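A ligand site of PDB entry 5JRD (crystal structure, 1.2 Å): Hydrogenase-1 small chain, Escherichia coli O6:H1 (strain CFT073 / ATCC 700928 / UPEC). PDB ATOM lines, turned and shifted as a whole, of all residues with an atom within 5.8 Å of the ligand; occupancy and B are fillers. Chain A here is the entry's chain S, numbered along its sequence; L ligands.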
ATOM      1  N   ILE A 186      -8.788  15.216  23.063  1.00  0.00           N
ATOM      2  CA  ILE A 186      -9.973  15.163  23.914  1.00  0.00           C
ATOM      3  C   ILE A 186     -10.732  16.508  23.891  1.00  0.00           C
ATOM      4  O   ILE A 186     -11.970  16.573  23.738  1.00  0.00           O
ATOM      5  CB  ILE A 186      -9.551  14.789  25.399  1.00  0.00           C
ATOM      6  CG1 ILE A 186      -9.027  13.350  25.522  1.00  0.00           C
ATOM      7  CG2 ILE A 186     -10.680  15.039  26.417  1.00  0.00           C
ATOM      8  CD1 ILE A 186      -9.990  12.292  25.211  1.00  0.00           C
ATOM      9  N   HIS A 187      -9.952  17.602  24.039  1.00  0.00           N
ATOM     10  CA  HIS A 187     -10.497  19.007  24.087  1.00  0.00           C
ATOM     11  C   HIS A 187     -11.107  19.481  22.785  1.00  0.00           C
ATOM     12  O   HIS A 187     -11.895  20.445  22.806  1.00  0.00           O
ATOM     13  CB  HIS A 187      -9.295  19.877  24.548  1.00  0.00           C
ATOM     14  CG  HIS A 187      -9.501  21.365  24.708  1.00  0.00           C
ATOM     15  ND1 HIS A 187     -10.173  21.966  25.766  1.00  0.00           N
ATOM     16  CD2 HIS A 187      -8.950  22.375  23.979  1.00  0.00           C
ATOM     17  CE1 HIS A 187     -10.056  23.287  25.632  1.00  0.00           C
ATOM     18  NE2 HIS A 187      -9.310  23.558  24.582  1.00  0.00           N
ATOM     19  N   CYS A 190     -14.804  17.885  23.169  1.00  0.00           N
ATOM     20  CA  CYS A 190     -15.351  17.865  24.550  1.00  0.00           C
ATOM     21  C   CYS A 190     -16.656  18.655  24.625  1.00  0.00           C
ATOM     22  O   CYS A 190     -16.740  19.847  24.233  1.00  0.00           O
ATOM     23  CB  CYS A 190     -14.321  18.442  25.555  1.00  0.00           C
ATOM     24  SG  CYS A 190     -14.925  18.411  27.294  1.00  0.00           S
ATOM     25  N   TYR A 191     -17.674  18.032  25.232  1.00  0.00           N
ATOM     26  CA  TYR A 191     -19.006  18.695  25.377  1.00  0.00           C
ATOM     27  C   TYR A 191     -19.020  19.875  26.358  1.00  0.00           C
ATOM     28  O   TYR A 191     -20.022  20.627  26.376  1.00  0.00           O
ATOM     29  CB  TYR A 191     -20.117  17.643  25.708  1.00  0.00           C
ATOM     30  CG  TYR A 191     -20.226  17.280  27.203  1.00  0.00           C
ATOM     31  CD1 TYR A 191     -19.138  16.808  27.973  1.00  0.00           C
ATOM     32  CD2 TYR A 191     -21.450  17.383  27.862  1.00  0.00           C
ATOM     33  CE1 TYR A 191     -19.274  16.498  29.328  1.00  0.00           C
ATOM     34  CE2 TYR A 191     -21.585  17.086  29.223  1.00  0.00           C
ATOM     35  CZ  TYR A 191     -20.502  16.645  29.976  1.00  0.00           C
ATOM     36  OH  TYR A 191     -20.580  16.424  31.337  1.00  0.00           O
ATOM     37  N   ARG A 192     -17.951  20.092  27.145  1.00  0.00           N
ATOM     38  CA  ARG A 192     -17.839  21.305  27.998  1.00  0.00           C
ATOM     39  C   ARG A 192     -17.090  22.450  27.301  1.00  0.00           C
ATOM     40  O   ARG A 192     -16.848  23.493  27.955  1.00  0.00           O
ATOM     41  CB  ARG A 192     -17.236  20.924  29.384  1.00  0.00           C
ATOM     42  CG  ARG A 192     -18.100  19.941  30.160  1.00  0.00           C
ATOM     43  CD  ARG A 192     -17.613  19.654  31.572  1.00  0.00           C
ATOM     44  NE  ARG A 192     -18.406  18.633  32.242  1.00  0.00           N
ATOM     45  CZ  ARG A 192     -18.574  18.493  33.552  1.00  0.00           C
ATOM     46  NH1 ARG A 192     -17.973  19.294  34.431  1.00  0.00           N
ATOM     47  NH2 ARG A 192     -19.312  17.456  34.006  1.00  0.00           N
ATOM     48  N   ARG A 193     -16.727  22.322  26.029  1.00  0.00           N
ATOM     49  CA  ARG A 193     -15.934  23.355  25.365  1.00  0.00           C
ATOM     50  C   ARG A 193     -16.648  24.711  25.330  1.00  0.00           C
ATOM     51  O   ARG A 193     -15.985  25.744  25.400  1.00  0.00           O
ATOM     52  CB  ARG A 193     -15.522  22.891  23.974  1.00  0.00           C
ATOM     53  CG  ARG A 193     -14.571  23.766  23.236  1.00  0.00           C
ATOM     54  CD  ARG A 193     -13.180  23.879  23.874  1.00  0.00           C
ATOM     55  NE  ARG A 193     -12.480  24.805  22.998  1.00  0.00           N
ATOM     56  CZ  ARG A 193     -11.652  24.504  22.009  1.00  0.00           C
ATOM     57  NH1 ARG A 193     -11.223  23.274  21.751  1.00  0.00           N
ATOM     58  NH2 ARG A 193     -11.212  25.502  21.263  1.00  0.00           N
ATOM     59  N   PHE A 196     -15.493  26.455  28.436  1.00  0.00           N
ATOM     60  CA  PHE A 196     -14.077  26.908  28.260  1.00  0.00           C
ATOM     61  C   PHE A 196     -14.066  28.220  27.475  1.00  0.00           C
ATOM     62  O   PHE A 196     -13.416  29.228  27.880  1.00  0.00           O
ATOM     63  CB  PHE A 196     -13.272  25.822  27.539  1.00  0.00           C
ATOM     64  CG  PHE A 196     -11.821  26.190  27.274  1.00  0.00           C
ATOM     65  CD1 PHE A 196     -10.827  25.908  28.212  1.00  0.00           C
ATOM     66  CD2 PHE A 196     -11.448  26.781  26.088  1.00  0.00           C
ATOM     67  CE1 PHE A 196      -9.492  26.222  27.937  1.00  0.00           C
ATOM     68  CE2 PHE A 196     -10.121  27.065  25.812  1.00  0.00           C
ATOM     69  CZ  PHE A 196      -9.133  26.814  26.733  1.00  0.00           C
ATOM     70  N   TYR A 214     -19.696  22.916  34.376  1.00  0.00           N
ATOM     71  CA  TYR A 214     -18.726  23.821  33.773  1.00  0.00           C
ATOM     72  C   TYR A 214     -17.369  23.174  33.525  1.00  0.00           C
ATOM     73  O   TYR A 214     -17.068  22.046  33.966  1.00  0.00           O
ATOM     74  CB  TYR A 214     -18.604  25.146  34.603  1.00  0.00           C
ATOM     75  CG  TYR A 214     -19.772  26.153  34.459  1.00  0.00           C
ATOM     76  CD1 TYR A 214     -20.961  25.856  33.765  1.00  0.00           C
ATOM     77  CD2 TYR A 214     -19.672  27.407  35.076  1.00  0.00           C
ATOM     78  CE1 TYR A 214     -22.001  26.792  33.648  1.00  0.00           C
ATOM     79  CE2 TYR A 214     -20.708  28.339  34.951  1.00  0.00           C
ATOM     80  CZ  TYR A 214     -21.872  28.022  34.265  1.00  0.00           C
ATOM     81  OH  TYR A 214     -22.873  28.994  34.183  1.00  0.00           O
ATOM     82  N   CYS A 215     -16.508  23.872  32.773  1.00  0.00           N
ATOM     83  CA  CYS A 215     -15.209  23.331  32.322  1.00  0.00           C
ATOM     84  C   CYS A 215     -14.272  23.120  33.509  1.00  0.00           C
ATOM     85  O   CYS A 215     -14.299  23.919  34.483  1.00  0.00           O
ATOM     86  CB  CYS A 215     -14.599  24.265  31.252  1.00  0.00           C
ATOM     87  SG  CYS A 215     -12.846  23.998  30.805  1.00  0.00           S
ATOM     88  N   LEU A 216     -13.437  22.085  33.387  1.00  0.00           N
ATOM     89  CA  LEU A 216     -12.493  21.608  34.441  1.00  0.00           C
ATOM     90  C   LEU A 216     -11.041  22.088  34.255  1.00  0.00           C
ATOM     91  O   LEU A 216     -10.128  21.645  34.975  1.00  0.00           O
ATOM     92  CB  LEU A 216     -12.592  20.090  34.543  1.00  0.00           C
ATOM     93  CG  LEU A 216     -14.000  19.620  34.954  1.00  0.00           C
ATOM     94  CD1 LEU A 216     -14.147  18.103  34.779  1.00  0.00           C
ATOM     95  CD2 LEU A 216     -14.436  19.973  36.352  1.00  0.00           C
ATOM     96  N   TYR A 217     -10.798  23.031  33.324  1.00  0.00           N
ATOM     97  CA  TYR A 217      -9.429  23.526  33.062  1.00  0.00           C
ATOM     98  C   TYR A 217      -8.693  24.063  34.306  1.00  0.00           C
ATOM     99  O   TYR A 217      -7.502  23.747  34.541  1.00  0.00           O
ATOM    100  CB  TYR A 217      -9.540  24.610  31.991  1.00  0.00           C
ATOM    101  CG  TYR A 217      -8.241  25.279  31.714  1.00  0.00           C
ATOM    102  CD1 TYR A 217      -7.224  24.617  31.027  1.00  0.00           C
ATOM    103  CD2 TYR A 217      -8.039  26.585  32.151  1.00  0.00           C
ATOM    104  CE1 TYR A 217      -6.055  25.215  30.776  1.00  0.00           C
ATOM    105  CE2 TYR A 217      -6.880  27.194  31.926  1.00  0.00           C
ATOM    106  CZ  TYR A 217      -5.867  26.516  31.256  1.00  0.00           C
ATOM    107  OH  TYR A 217      -4.789  27.153  31.044  1.00  0.00           O
ATOM    108  N   CYS A 221      -7.490  19.928  34.287  1.00  0.00           N
ATOM    109  CA  CYS A 221      -7.796  19.042  33.123  1.00  0.00           C
ATOM    110  C   CYS A 221      -6.671  19.117  32.048  1.00  0.00           C
ATOM    111  O   CYS A 221      -6.327  20.222  31.578  1.00  0.00           O
ATOM    112  CB  CYS A 221      -9.117  19.504  32.473  1.00  0.00           C
ATOM    113  SG  CYS A 221      -9.664  18.395  31.135  1.00  0.00           S
ATOM    114  N   LYS A 222      -6.176  17.936  31.630  1.00  0.00           N
ATOM    115  CA  LYS A 222      -5.134  17.832  30.592  1.00  0.00           C
ATOM    116  C   LYS A 222      -5.709  17.500  29.204  1.00  0.00           C
ATOM    117  O   LYS A 222      -4.942  17.174  28.271  1.00  0.00           O
ATOM    118  CB  LYS A 222      -4.036  16.858  31.032  1.00  0.00           C
ATOM    119  CG  LYS A 222      -3.362  17.260  32.382  1.00  0.00           C
ATOM    120  CD  LYS A 222      -2.914  18.727  32.411  1.00  0.00           C
ATOM    121  CE  LYS A 222      -2.085  19.235  33.577  1.00  0.00           C
ATOM    122  NZ  LYS A 222      -2.619  18.846  34.909  1.00  0.00           N
ATOM    123  N   GLY A 223      -7.033  17.592  29.051  1.00  0.00           N
ATOM    124  CA  GLY A 223      -7.650  17.393  27.748  1.00  0.00           C
ATOM    125  C   GLY A 223      -7.028  18.168  26.569  1.00  0.00           C
ATOM    126  O   GLY A 223      -6.921  17.642  25.445  1.00  0.00           O
ATOM    127  N   PRO A 224      -6.580  19.430  26.833  1.00  0.00           N
ATOM    128  CA  PRO A 224      -5.983  20.220  25.707  1.00  0.00           C
ATOM    129  C   PRO A 224      -4.713  19.641  25.074  1.00  0.00           C
ATOM    130  O   PRO A 224      -4.376  20.055  23.966  1.00  0.00           O
ATOM    131  CB  PRO A 224      -5.708  21.602  26.374  1.00  0.00           C
ATOM    132  CG  PRO A 224      -6.792  21.706  27.383  1.00  0.00           C
ATOM    133  CD  PRO A 224      -6.886  20.321  27.978  1.00  0.00           C
ATOM    134  N   ILE A 243     -14.280  13.432  32.436  1.00  0.00           N
ATOM    135  CA  ILE A 243     -14.785  14.821  32.531  1.00  0.00           C
ATOM    136  C   ILE A 243     -16.300  14.797  32.753  1.00  0.00           C
ATOM    137  O   ILE A 243     -16.813  15.661  33.508  1.00  0.00           O
ATOM    138  CB  ILE A 243     -14.366  15.577  31.242  1.00  0.00           C
ATOM    139  CG1 ILE A 243     -12.855  15.905  31.255  1.00  0.00           C
ATOM    140  CG2 ILE A 243     -15.204  16.831  30.968  1.00  0.00           C
ATOM    141  CD1 ILE A 243     -12.197  15.910  29.880  1.00  0.00           C
ATOM    142  N   CYS A 249      -9.357  15.348  32.845  1.00  0.00           N
ATOM    143  CA  CYS A 249      -8.459  14.362  32.222  1.00  0.00           C
ATOM    144  C   CYS A 249      -7.075  14.445  32.942  1.00  0.00           C
ATOM    145  O   CYS A 249      -6.576  15.560  33.247  1.00  0.00           O
ATOM    146  CB  CYS A 249      -8.380  14.684  30.698  1.00  0.00           C
ATOM    147  SG  CYS A 249      -7.179  13.702  29.716  1.00  0.00           S
HETATM  148 FE1  LIG L   1     -12.584  22.044  29.623  1.00  0.00          FE
HETATM  149 FE2  LIG L   1     -11.039  19.736  29.825  1.00  0.00          FE
HETATM  150 FE3  LIG L   1     -11.132  21.180  27.469  1.00  0.00          FE
HETATM  151 FE4  LIG L   1     -13.320  19.749  28.258  1.00  0.00          FE
HETATM  152  S1  LIG L   1     -11.207  18.904  27.683  1.00  0.00           S
HETATM  153  S2  LIG L   1     -13.351  21.920  27.450  1.00  0.00           S
HETATM  154  S3  LIG L   1     -13.256  20.040  30.559  1.00  0.00           S
HETATM  155  S4  LIG L   1     -10.244  21.862  29.484  1.00  0.00           S
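The side-chain sulfur (SG) of Cys 215 is bound to an iron atom (FE1) of the ligand (2.3 Å).
N of Arg 193 sits close to S2 of the ligand (3.7 Å).
The side-chain sulfur (SG) of Cys 221 is bound to an iron atom (FE2) of the ligand, 2.3 Å away.
N of Leu 216 sits close to S3 of the ligand.
The side-chain sulfur (SG) of Cys 190 is bound to an iron atom (FE4) of the ligand (2.3 Å).
ND1 of His 187 binds FE3 of the ligand, 2.1 Å away.
The backbone NH (N) of Tyr 217 lies close to the side-chain sulfur (SG) of Cys 215 (3.4 Å).
The backbone carbonyl oxygen of Leu 216 lies within hydrogen-bond range of the backbone NH of Cys 221, 3.2 Å away.
The backbone carbonyl oxygen (O) of Tyr 214 sits at hydrogen-bond distance from the guanidinium group (NH1) of Arg 192 (2.9 Å).
NH2 of Arg 192 lies within hydrogen-bond range of O of Ile 243, 3.1 Å away.
The backbone carbonyl oxygen (O) of His 187 sits at hydrogen-bond distance from the guanidinium group (NH1) of Arg 193.
N of Gly 223 lies close to SG of Cys 221 (3.5 Å).
SG of Cys 221 sits close to N of Cys 249 (3.5 Å).
N of His 187 sits at hydrogen-bond distance from O of Gly 223.
Arg 192 touches the ligand (C to S2, 3.8 Å).
Phe 196 touches the ligand (CB to S2, 3.9 Å).
CB of Tyr 217 touches S4 of the ligand, at 3.8 Å.
Gly 223 touches the ligand (CA to S1, 3.9 Å).
Pro 224 touches the ligand.
Ile 243 touches the ligand (CG2 to S3, 3.8 Å).
Hydrophobic or aromatic side chains that line the ligand: His 187, Phe 196, Tyr 217, Pro 224 and Ile 243.
Within 4 Å of the ligand: His 187, Cys 190, Arg 192, Arg 193, Phe 196, Cys 215, Leu 216, Tyr 217, Cys 221, Gly 223, Pro 224 and Ile 243.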
